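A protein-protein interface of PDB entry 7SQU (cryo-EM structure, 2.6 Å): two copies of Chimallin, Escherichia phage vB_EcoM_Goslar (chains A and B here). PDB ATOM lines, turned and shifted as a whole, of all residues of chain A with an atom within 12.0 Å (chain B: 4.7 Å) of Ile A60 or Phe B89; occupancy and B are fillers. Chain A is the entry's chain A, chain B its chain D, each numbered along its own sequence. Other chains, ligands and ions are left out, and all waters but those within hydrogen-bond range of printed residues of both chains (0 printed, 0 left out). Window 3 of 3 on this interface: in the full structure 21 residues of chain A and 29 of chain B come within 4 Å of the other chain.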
ATOM      1  N   ASN A  53      -0.036  -2.750  -3.645  1.00  0.00           N
ATOM      2  CA  ASN A  53      -1.330  -2.532  -4.285  1.00  0.00           C
ATOM      3  C   ASN A  53      -1.536  -3.453  -5.481  1.00  0.00           C
ATOM      4  O   ASN A  53      -2.653  -3.908  -5.729  1.00  0.00           O
ATOM      5  CB  ASN A  53      -1.499  -1.067  -4.662  1.00  0.00           C
ATOM      6  CG  ASN A  53      -1.796  -0.198  -3.461  1.00  0.00           C
ATOM      7  OD1 ASN A  53      -2.079  -0.698  -2.381  1.00  0.00           O
ATOM      8  ND2 ASN A  53      -1.729   1.106  -3.641  1.00  0.00           N
ATOM      9  N   ARG A  54      -0.487  -3.699  -6.269  1.00  0.00           N
ATOM     10  CA  ARG A  54      -0.608  -4.650  -7.370  1.00  0.00           C
ATOM     11  C   ARG A  54      -0.851  -6.070  -6.873  1.00  0.00           C
ATOM     12  O   ARG A  54      -1.613  -6.820  -7.489  1.00  0.00           O
ATOM     13  CB  ARG A  54       0.618  -4.597  -8.270  1.00  0.00           C
ATOM     14  CG  ARG A  54       0.808  -3.257  -8.916  1.00  0.00           C
ATOM     15  CD  ARG A  54       2.024  -3.224  -9.818  1.00  0.00           C
ATOM     16  NE  ARG A  54       3.186  -3.908  -9.261  1.00  0.00           N
ATOM     17  CZ  ARG A  54       3.607  -5.105  -9.652  1.00  0.00           C
ATOM     18  NH1 ARG A  54       2.983  -5.780 -10.601  1.00  0.00           N
ATOM     19  NH2 ARG A  54       4.684  -5.632  -9.079  1.00  0.00           N
ATOM     20  N   LEU A  56      -2.187  -7.127  -3.656  1.00  0.00           N
ATOM     21  CA  LEU A  56      -3.524  -7.111  -3.065  1.00  0.00           C
ATOM     22  C   LEU A  56      -4.297  -5.949  -3.682  1.00  0.00           C
ATOM     23  O   LEU A  56      -4.319  -4.846  -3.146  1.00  0.00           O
ATOM     24  CB  LEU A  56      -3.433  -6.987  -1.550  1.00  0.00           C
ATOM     25  CG  LEU A  56      -2.340  -7.798  -0.860  1.00  0.00           C
ATOM     26  CD1 LEU A  56      -2.270  -7.470   0.611  1.00  0.00           C
ATOM     27  CD2 LEU A  56      -2.593  -9.273  -1.040  1.00  0.00           C
ATOM     28  N   SER A  57      -4.948  -6.192  -4.814  1.00  0.00           N
ATOM     29  CA  SER A  57      -5.567  -5.118  -5.580  1.00  0.00           C
ATOM     30  C   SER A  57      -7.070  -5.026  -5.348  1.00  0.00           C
ATOM     31  O   SER A  57      -7.723  -5.980  -4.928  1.00  0.00           O
ATOM     32  CB  SER A  57      -5.290  -5.299  -7.071  1.00  0.00           C
ATOM     33  OG  SER A  57      -5.753  -6.550  -7.526  1.00  0.00           O
ATOM     34  N   ARG A  58      -7.613  -3.843  -5.649  1.00  0.00           N
ATOM     35  CA  ARG A  58      -9.040  -3.570  -5.602  1.00  0.00           C
ATOM     36  C   ARG A  58      -9.443  -2.808  -6.857  1.00  0.00           C
ATOM     37  O   ARG A  58      -8.634  -2.098  -7.453  1.00  0.00           O
ATOM     38  CB  ARG A  58      -9.402  -2.770  -4.349  1.00  0.00           C
ATOM     39  CG  ARG A  58      -9.180  -3.520  -3.053  1.00  0.00           C
ATOM     40  CD  ARG A  58     -10.154  -4.651  -2.902  1.00  0.00           C
ATOM     41  NE  ARG A  58     -10.059  -5.320  -1.614  1.00  0.00           N
ATOM     42  CZ  ARG A  58      -9.456  -6.482  -1.429  1.00  0.00           C
ATOM     43  NH1 ARG A  58      -8.855  -7.111  -2.418  1.00  0.00           N
ATOM     44  NH2 ARG A  58      -9.475  -7.038  -0.225  1.00  0.00           N
ATOM     45  N   ARG A  59     -10.708  -2.957  -7.259  1.00  0.00           N
ATOM     46  CA  ARG A  59     -11.157  -2.391  -8.529  1.00  0.00           C
ATOM     47  C   ARG A  59     -11.326  -0.877  -8.473  1.00  0.00           C
ATOM     48  O   ARG A  59     -10.960  -0.182  -9.423  1.00  0.00           O
ATOM     49  CB  ARG A  59     -12.461  -3.047  -8.972  1.00  0.00           C
ATOM     50  CG  ARG A  59     -12.283  -4.419  -9.571  1.00  0.00           C
ATOM     51  CD  ARG A  59     -13.608  -5.051  -9.922  1.00  0.00           C
ATOM     52  NE  ARG A  59     -14.405  -5.304  -8.732  1.00  0.00           N
ATOM     53  CZ  ARG A  59     -15.368  -6.208  -8.651  1.00  0.00           C
ATOM     54  NH1 ARG A  59     -15.683  -6.976  -9.677  1.00  0.00           N
ATOM     55  NH2 ARG A  59     -16.033  -6.346  -7.507  1.00  0.00           N
ATOM     56  N   ILE A  60     -11.879  -0.345  -7.389  1.00  0.00           N
ATOM     57  CA  ILE A  60     -12.143   1.084  -7.261  1.00  0.00           C
ATOM     58  C   ILE A  60     -11.270   1.640  -6.148  1.00  0.00           C
ATOM     59  O   ILE A  60     -11.308   1.137  -5.021  1.00  0.00           O
ATOM     60  CB  ILE A  60     -13.627   1.364  -6.975  1.00  0.00           C
ATOM     61  CG1 ILE A  60     -14.473   1.117  -8.217  1.00  0.00           C
ATOM     62  CG2 ILE A  60     -13.817   2.785  -6.515  1.00  0.00           C
ATOM     63  CD1 ILE A  60     -15.174  -0.186  -8.207  1.00  0.00           C
ATOM     64  N   SER A  61     -10.510   2.686  -6.451  1.00  0.00           N
ATOM     65  CA  SER A  61      -9.567   3.257  -5.505  1.00  0.00           C
ATOM     66  C   SER A  61      -9.948   4.678  -5.117  1.00  0.00           C
ATOM     67  O   SER A  61     -10.471   5.448  -5.923  1.00  0.00           O
ATOM     68  CB  SER A  61      -8.155   3.261  -6.074  1.00  0.00           C
ATOM     69  OG  SER A  61      -7.996   4.335  -6.978  1.00  0.00           O
ATOM     70  N   ARG A  62      -9.716   5.023  -3.845  1.00  0.00           N
ATOM     71  CA  ARG A  62     -10.122   6.361  -3.331  1.00  0.00           C
ATOM     72  C   ARG A  62      -9.026   7.393  -3.620  1.00  0.00           C
ATOM     73  O   ARG A  62      -9.353   8.593  -3.693  1.00  0.00           O
ATOM     74  CB  ARG A  62     -10.399   6.283  -1.826  1.00  0.00           C
ATOM     75  CG  ARG A  62     -11.210   5.067  -1.403  1.00  0.00           C
ATOM     76  CD  ARG A  62     -11.162   4.870   0.099  1.00  0.00           C
ATOM     77  NE  ARG A  62      -9.796   4.807   0.599  1.00  0.00           N
ATOM     78  CZ  ARG A  62      -9.092   3.690   0.745  1.00  0.00           C
ATOM     79  NH1 ARG A  62      -9.626   2.523   0.429  1.00  0.00           N
ATOM     80  NH2 ARG A  62      -7.856   3.745   1.206  1.00  0.00           N
ATOM     81  N   ASN A  63      -7.780   6.940  -3.775  1.00  0.00           N
ATOM     82  CA  ASN A  63      -6.654   7.867  -4.073  1.00  0.00           C
ATOM     83  C   ASN A  63      -6.211   7.680  -5.530  1.00  0.00           C
ATOM     84  O   ASN A  63      -5.799   6.559  -5.884  1.00  0.00           O
ATOM     85  CB  ASN A  63      -5.509   7.703  -3.069  1.00  0.00           C
ATOM     86  CG  ASN A  63      -5.330   6.286  -2.560  1.00  0.00           C
ATOM     87  OD1 ASN A  63      -5.675   5.320  -3.238  1.00  0.00           O
ATOM     88  ND2 ASN A  63      -4.775   6.150  -1.368  1.00  0.00           N
ATOM     89  N   THR A  64      -6.311   8.736  -6.344  1.00  0.00           N
ATOM     90  CA  THR A  64      -5.954   8.633  -7.786  1.00  0.00           C
ATOM     91  C   THR A  64      -4.762   9.538  -8.120  1.00  0.00           C
ATOM     92  O   THR A  64      -4.120   9.296  -9.161  1.00  0.00           O
ATOM     93  CB  THR A  64      -7.157   8.972  -8.676  1.00  0.00           C
ATOM     94  OG1 THR A  64      -7.566  10.306  -8.369  1.00  0.00           O
ATOM     95  CG2 THR A  64      -8.319   8.022  -8.482  1.00  0.00           C
ATOM     96  N   GLY A  65      -4.480  10.539  -7.279  1.00  0.00           N
ATOM     97  CA  GLY A  65      -3.385  11.490  -7.558  1.00  0.00           C
ATOM     98  C   GLY A  65      -3.814  12.603  -8.502  1.00  0.00           C
ATOM     99  O   GLY A  65      -5.006  12.636  -8.867  1.00  0.00           O
ATOM    100  N   TYR B  79     -20.496   7.483 -12.482  1.00  0.00           N
ATOM    101  CA  TYR B  79     -19.073   7.306 -12.222  1.00  0.00           C
ATOM    102  C   TYR B  79     -18.526   6.085 -12.941  1.00  0.00           C
ATOM    103  O   TYR B  79     -17.409   6.112 -13.461  1.00  0.00           O
ATOM    104  CB  TYR B  79     -18.810   7.179 -10.729  1.00  0.00           C
ATOM    105  CG  TYR B  79     -17.396   6.780 -10.401  1.00  0.00           C
ATOM    106  CD1 TYR B  79     -16.393   7.724 -10.324  1.00  0.00           C
ATOM    107  CD2 TYR B  79     -17.063   5.461 -10.182  1.00  0.00           C
ATOM    108  CE1 TYR B  79     -15.105   7.366 -10.032  1.00  0.00           C
ATOM    109  CE2 TYR B  79     -15.776   5.093  -9.896  1.00  0.00           C
ATOM    110  CZ  TYR B  79     -14.803   6.049  -9.817  1.00  0.00           C
ATOM    111  OH  TYR B  79     -13.516   5.682  -9.525  1.00  0.00           O
ATOM    112  N   LEU B  80     -19.281   4.991 -12.950  1.00  0.00           N
ATOM    113  CA  LEU B  80     -18.767   3.755 -13.531  1.00  0.00           C
ATOM    114  C   LEU B  80     -18.796   3.731 -15.049  1.00  0.00           C
ATOM    115  O   LEU B  80     -18.103   2.906 -15.645  1.00  0.00           O
ATOM    116  CB  LEU B  80     -19.565   2.560 -13.027  1.00  0.00           C
ATOM    117  CG  LEU B  80     -19.085   1.853 -11.773  1.00  0.00           C
ATOM    118  CD1 LEU B  80     -20.129   0.866 -11.351  1.00  0.00           C
ATOM    119  CD2 LEU B  80     -17.775   1.165 -12.014  1.00  0.00           C
ATOM    120  N   PHE B  85     -15.119  -1.307 -15.709  1.00  0.00           N
ATOM    121  CA  PHE B  85     -15.875  -2.172 -14.811  1.00  0.00           C
ATOM    122  C   PHE B  85     -17.368  -1.886 -14.905  1.00  0.00           C
ATOM    123  O   PHE B  85     -18.087  -1.932 -13.913  1.00  0.00           O
ATOM    124  CB  PHE B  85     -15.399  -2.018 -13.374  1.00  0.00           C
ATOM    125  CG  PHE B  85     -13.936  -2.171 -13.219  1.00  0.00           C
ATOM    126  CD1 PHE B  85     -13.335  -3.390 -13.434  1.00  0.00           C
ATOM    127  CD2 PHE B  85     -13.156  -1.096 -12.864  1.00  0.00           C
ATOM    128  CE1 PHE B  85     -11.977  -3.531 -13.296  1.00  0.00           C
ATOM    129  CE2 PHE B  85     -11.807  -1.232 -12.725  1.00  0.00           C
ATOM    130  CZ  PHE B  85     -11.215  -2.451 -12.940  1.00  0.00           C
ATOM    131  N   LYS B  86     -17.849  -1.596 -16.111  1.00  0.00           N
ATOM    132  CA  LYS B  86     -19.257  -1.273 -16.282  1.00  0.00           C
ATOM    133  C   LYS B  86     -20.150  -2.461 -15.954  1.00  0.00           C
ATOM    134  O   LYS B  86     -21.219  -2.294 -15.361  1.00  0.00           O
ATOM    135  CB  LYS B  86     -19.508  -0.791 -17.709  1.00  0.00           C
ATOM    136  CG  LYS B  86     -20.809  -0.023 -17.900  1.00  0.00           C
ATOM    137  CD  LYS B  86     -21.227   0.705 -16.634  1.00  0.00           C
ATOM    138  CE  LYS B  86     -22.310   1.733 -16.898  1.00  0.00           C
ATOM    139  NZ  LYS B  86     -22.797   2.336 -15.632  1.00  0.00           N
ATOM    140  N   ASP B  87     -19.737  -3.667 -16.329  1.00  0.00           N
ATOM    141  CA  ASP B  87     -20.574  -4.849 -16.205  1.00  0.00           C
ATOM    142  C   ASP B  87     -20.299  -5.671 -14.953  1.00  0.00           C
ATOM    143  O   ASP B  87     -20.865  -6.755 -14.808  1.00  0.00           O
ATOM    144  CB  ASP B  87     -20.420  -5.723 -17.441  1.00  0.00           C
ATOM    145  CG  ASP B  87     -20.235  -4.913 -18.696  1.00  0.00           C
ATOM    146  OD1 ASP B  87     -21.125  -4.098 -19.005  1.00  0.00           O
ATOM    147  OD2 ASP B  87     -19.204  -5.090 -19.375  1.00  0.00           O
ATOM    148  N   ASP B  88     -19.450  -5.198 -14.055  1.00  0.00           N
ATOM    149  CA  ASP B  88     -19.125  -5.971 -12.870  1.00  0.00           C
ATOM    150  C   ASP B  88     -20.077  -5.747 -11.706  1.00  0.00           C
ATOM    151  O   ASP B  88     -20.016  -6.500 -10.737  1.00  0.00           O
ATOM    152  CB  ASP B  88     -17.702  -5.661 -12.410  1.00  0.00           C
ATOM    153  CG  ASP B  88     -16.672  -6.515 -13.101  1.00  0.00           C
ATOM    154  OD1 ASP B  88     -16.906  -6.903 -14.260  1.00  0.00           O
ATOM    155  OD2 ASP B  88     -15.633  -6.811 -12.481  1.00  0.00           O
ATOM    156  N   PHE B  89     -20.967  -4.766 -11.780  1.00  0.00           N
ATOM    157  CA  PHE B  89     -21.824  -4.422 -10.658  1.00  0.00           C
ATOM    158  C   PHE B  89     -23.286  -4.466 -11.066  1.00  0.00           C
ATOM    159  O   PHE B  89     -23.640  -4.214 -12.216  1.00  0.00           O
ATOM    160  CB  PHE B  89     -21.494  -3.042 -10.116  1.00  0.00           C
ATOM    161  CG  PHE B  89     -20.145  -2.950  -9.493  1.00  0.00           C
ATOM    162  CD1 PHE B  89     -19.958  -3.261  -8.167  1.00  0.00           C
ATOM    163  CD2 PHE B  89     -19.059  -2.540 -10.232  1.00  0.00           C
ATOM    164  CE1 PHE B  89     -18.714  -3.173  -7.598  1.00  0.00           C
ATOM    165  CE2 PHE B  89     -17.820  -2.452  -9.663  1.00  0.00           C
ATOM    166  CZ  PHE B  89     -17.648  -2.768  -8.345  1.00  0.00           C
ATOM    167  N   ILE B  90     -24.124  -4.827 -10.103  1.00  0.00           N
ATOM    168  CA  ILE B  90     -25.571  -4.856 -10.253  1.00  0.00           C
ATOM    169  C   ILE B  90     -26.169  -4.053  -9.112  1.00  0.00           C
ATOM    170  O   ILE B  90     -25.775  -4.230  -7.959  1.00  0.00           O
ATOM    171  CB  ILE B  90     -26.112  -6.295 -10.235  1.00  0.00           C
ATOM    172  CG1 ILE B  90     -25.444  -7.121 -11.322  1.00  0.00           C
ATOM    173  CG2 ILE B  90     -27.601  -6.313 -10.418  1.00  0.00           C
ATOM    174  CD1 ILE B  90     -25.769  -8.578 -11.245  1.00  0.00           C
ATOM    175  N   PHE B  91     -27.106  -3.170  -9.427  1.00  0.00           N
ATOM    176  CA  PHE B  91     -27.747  -2.326  -8.430  1.00  0.00           C
ATOM    177  C   PHE B  91     -29.197  -2.751  -8.272  1.00  0.00           C
ATOM    178  O   PHE B  91     -29.931  -2.835  -9.257  1.00  0.00           O
ATOM    179  CB  PHE B  91     -27.656  -0.852  -8.814  1.00  0.00           C
ATOM    180  CG  PHE B  91     -26.256  -0.348  -8.919  1.00  0.00           C
ATOM    181  CD1 PHE B  91     -25.504  -0.116  -7.793  1.00  0.00           C
ATOM    182  CD2 PHE B  91     -25.684  -0.123 -10.146  1.00  0.00           C
ATOM    183  CE1 PHE B  91     -24.216   0.338  -7.893  1.00  0.00           C
ATOM    184  CE2 PHE B  91     -24.403   0.336 -10.245  1.00  0.00           C
ATOM    185  CZ  PHE B  91     -23.669   0.563  -9.117  1.00  0.00           C
ATOM    186  N   VAL B 108     -25.735  -3.188  -3.584  1.00  0.00           N
ATOM    187  CA  VAL B 108     -24.673  -3.281  -4.582  1.00  0.00           C
ATOM    188  C   VAL B 108     -24.166  -4.716  -4.607  1.00  0.00           C
ATOM    189  O   VAL B 108     -23.677  -5.220  -3.595  1.00  0.00           O
ATOM    190  CB  VAL B 108     -23.525  -2.311  -4.270  1.00  0.00           C
ATOM    191  CG1 VAL B 108     -22.513  -2.305  -5.385  1.00  0.00           C
ATOM    192  CG2 VAL B 108     -24.060  -0.924  -4.033  1.00  0.00           C
ATOM    193  N   MET B 109     -24.249  -5.366  -5.764  1.00  0.00           N
ATOM    194  CA  MET B 109     -23.931  -6.779  -5.895  1.00  0.00           C
ATOM    195  C   MET B 109     -22.786  -7.002  -6.870  1.00  0.00           C
ATOM    196  O   MET B 109     -22.618  -6.258  -7.834  1.00  0.00           O
ATOM    197  CB  MET B 109     -25.142  -7.570  -6.369  1.00  0.00           C
ATOM    198  CG  MET B 109     -26.014  -8.086  -5.273  1.00  0.00           C
ATOM    199  SD  MET B 109     -27.223  -9.299  -5.818  1.00  0.00           S
ATOM    200  CE  MET B 109     -27.355  -8.909  -7.543  1.00  0.00           C
ATOM    201  N   SER B 110     -22.007  -8.052  -6.614  1.00  0.00           N
ATOM    202  CA  SER B 110     -20.961  -8.495  -7.522  1.00  0.00           C
ATOM    203  C   SER B 110     -20.764  -9.994  -7.331  1.00  0.00           C
ATOM    204  O   SER B 110     -21.146 -10.554  -6.304  1.00  0.00           O
ATOM    205  CB  SER B 110     -19.664  -7.724  -7.303  1.00  0.00           C
ATOM    206  OG  SER B 110     -18.729  -8.037  -8.305  1.00  0.00           O
ATOM    207  N   LEU B 204     -19.107   3.604  -2.902  1.00  0.00           N
ATOM    208  CA  LEU B 204     -18.823   2.536  -3.853  1.00  0.00           C
ATOM    209  C   LEU B 204     -17.497   1.857  -3.543  1.00  0.00           C
ATOM    210  O   LEU B 204     -17.383   0.628  -3.627  1.00  0.00           O
ATOM    211  CB  LEU B 204     -18.824   3.095  -5.272  1.00  0.00           C
ATOM    212  CG  LEU B 204     -18.735   2.097  -6.416  1.00  0.00           C
ATOM    213  CD1 LEU B 204     -19.914   1.170  -6.412  1.00  0.00           C
ATOM    214  CD2 LEU B 204     -18.659   2.823  -7.723  1.00  0.00           C
ATOM    215  N   SER B 205     -16.479   2.637  -3.184  1.00  0.00           N
ATOM    216  CA  SER B 205     -15.193   2.044  -2.832  1.00  0.00           C
ATOM    217  C   SER B 205     -15.308   1.138  -1.610  1.00  0.00           C
ATOM    218  O   SER B 205     -14.717   0.048  -1.572  1.00  0.00           O
ATOM    219  CB  SER B 205     -14.168   3.141  -2.592  1.00  0.00           C
ATOM    220  OG  SER B 205     -12.916   2.581  -2.278  1.00  0.00           O
ATOM    221  N   ASP B 208     -16.969  -2.162  -2.611  1.00  0.00           N
ATOM    222  CA  ASP B 208     -16.067  -3.016  -3.373  1.00  0.00           C
ATOM    223  C   ASP B 208     -15.054  -3.712  -2.473  1.00  0.00           C
ATOM    224  O   ASP B 208     -14.802  -4.912  -2.627  1.00  0.00           O
ATOM    225  CB  ASP B 208     -15.364  -2.183  -4.438  1.00  0.00           C
ATOM    226  CG  ASP B 208     -14.274  -2.943  -5.148  1.00  0.00           C
ATOM    227  OD1 ASP B 208     -14.561  -4.021  -5.699  1.00  0.00           O
ATOM    228  OD2 ASP B 208     -13.127  -2.461  -5.166  1.00  0.00           O
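The guanidinium group (NH1) of Arg A59 is in salt-bridge range of the side-chain carboxylate (OD2) of Asp B88 (2.8 Å). The guanidinium group (NH2) of Arg A59 sits at hydrogen-bond distance from the side-chain hydroxyl (OG) of Ser B110 (3.3 Å). NH2 of Arg A59 is in salt-bridge range of OD1 of Asp B208 (3.3 Å). The backbone carbonyl oxygen (O) of Ile A60 sits at hydrogen-bond distance from the side-chain hydroxyl (OG) of Ser B205, at 3.5 Å. The side-chain carboxylate of Asp B208 is in hydrogen-bond range of the backbone NH of Ile A60 (3.3 Å).
O of Asp B88 lies within hydrogen-bond range of OG of Ser B110 (3.2 Å).
CB of Arg A58 touches OD2 of Asp B208, at 3.8 Å. O of Arg A59 touches CE2 of Phe B85 (3.6 Å). Phe B89 touches Ile A60 (CZ to CD1, 3.6 Å). OG of Ser B205 touches CG of Arg A62 (3.1 Å).
Asn A53 touches none of the printed residues of chain B. Ser A57 touches none of the printed residues of chain B. Of the printed residues of chain B, Arg A58 touches Asp B208 (3.8 Å). Printed residues of chain B within 4 Å of Arg A59: Phe B85, Asp B88, Ser B110 and Asp B208. Of chain B, only Phe B89 (3.6 Å), Ser B205 (3.5 Å) and Asp B208 (3.3 Å) come within 4 Å of Ile A60. Printed residues of chain B within 4 Å of Arg A62: Ser B205. No residue of chain A comes within 4 Å of Leu B80. Of the printed residues of chain A, Phe B85 touches Arg A59. No residue of chain A comes within 4 Å of Asp B87. Of the printed residues of chain A, Phe B89 touches Ile A60. No residue of chain A comes within 4 Å of Ile B90. No residue of chain A comes within 4 Å of Phe B91. No residue of chain A comes within 4 Å of Val B108. Ser B110 touches one residue of chain A. Ser B205 touches just these residues of chain A: Ile A60 and Arg A62. Asp B208 touches three residues of chain A. The nearest residue of chain B that does not touch Ile A60 is Tyr B79 (4.2 Å). The nearest printed residue of chain A that does not touch Phe B89 is Arg A59 (4.01 Å).
Hydrophobic or aromatic side chains of chain B within 4 Å of the printed part of chain A: Phe B85 and Phe B89. Of the 12 printed residues of chain A, 4 touch a printed residue of chain B. Hydrophobic or aromatic side chains of chain A within 4 Å of the printed part of chain B: Ile A60. Among the printed residues, 9 pairs touch across the chains. Among the printed residues, Asp or Glu carboxylates within 4 Å of a Lys or Arg side-chain nitrogen of the other chain: Arg A59 with Asp B88 (2.8 Å) and Arg A59 with Asp B208 (3.3 Å).
No position is printed for both chains.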
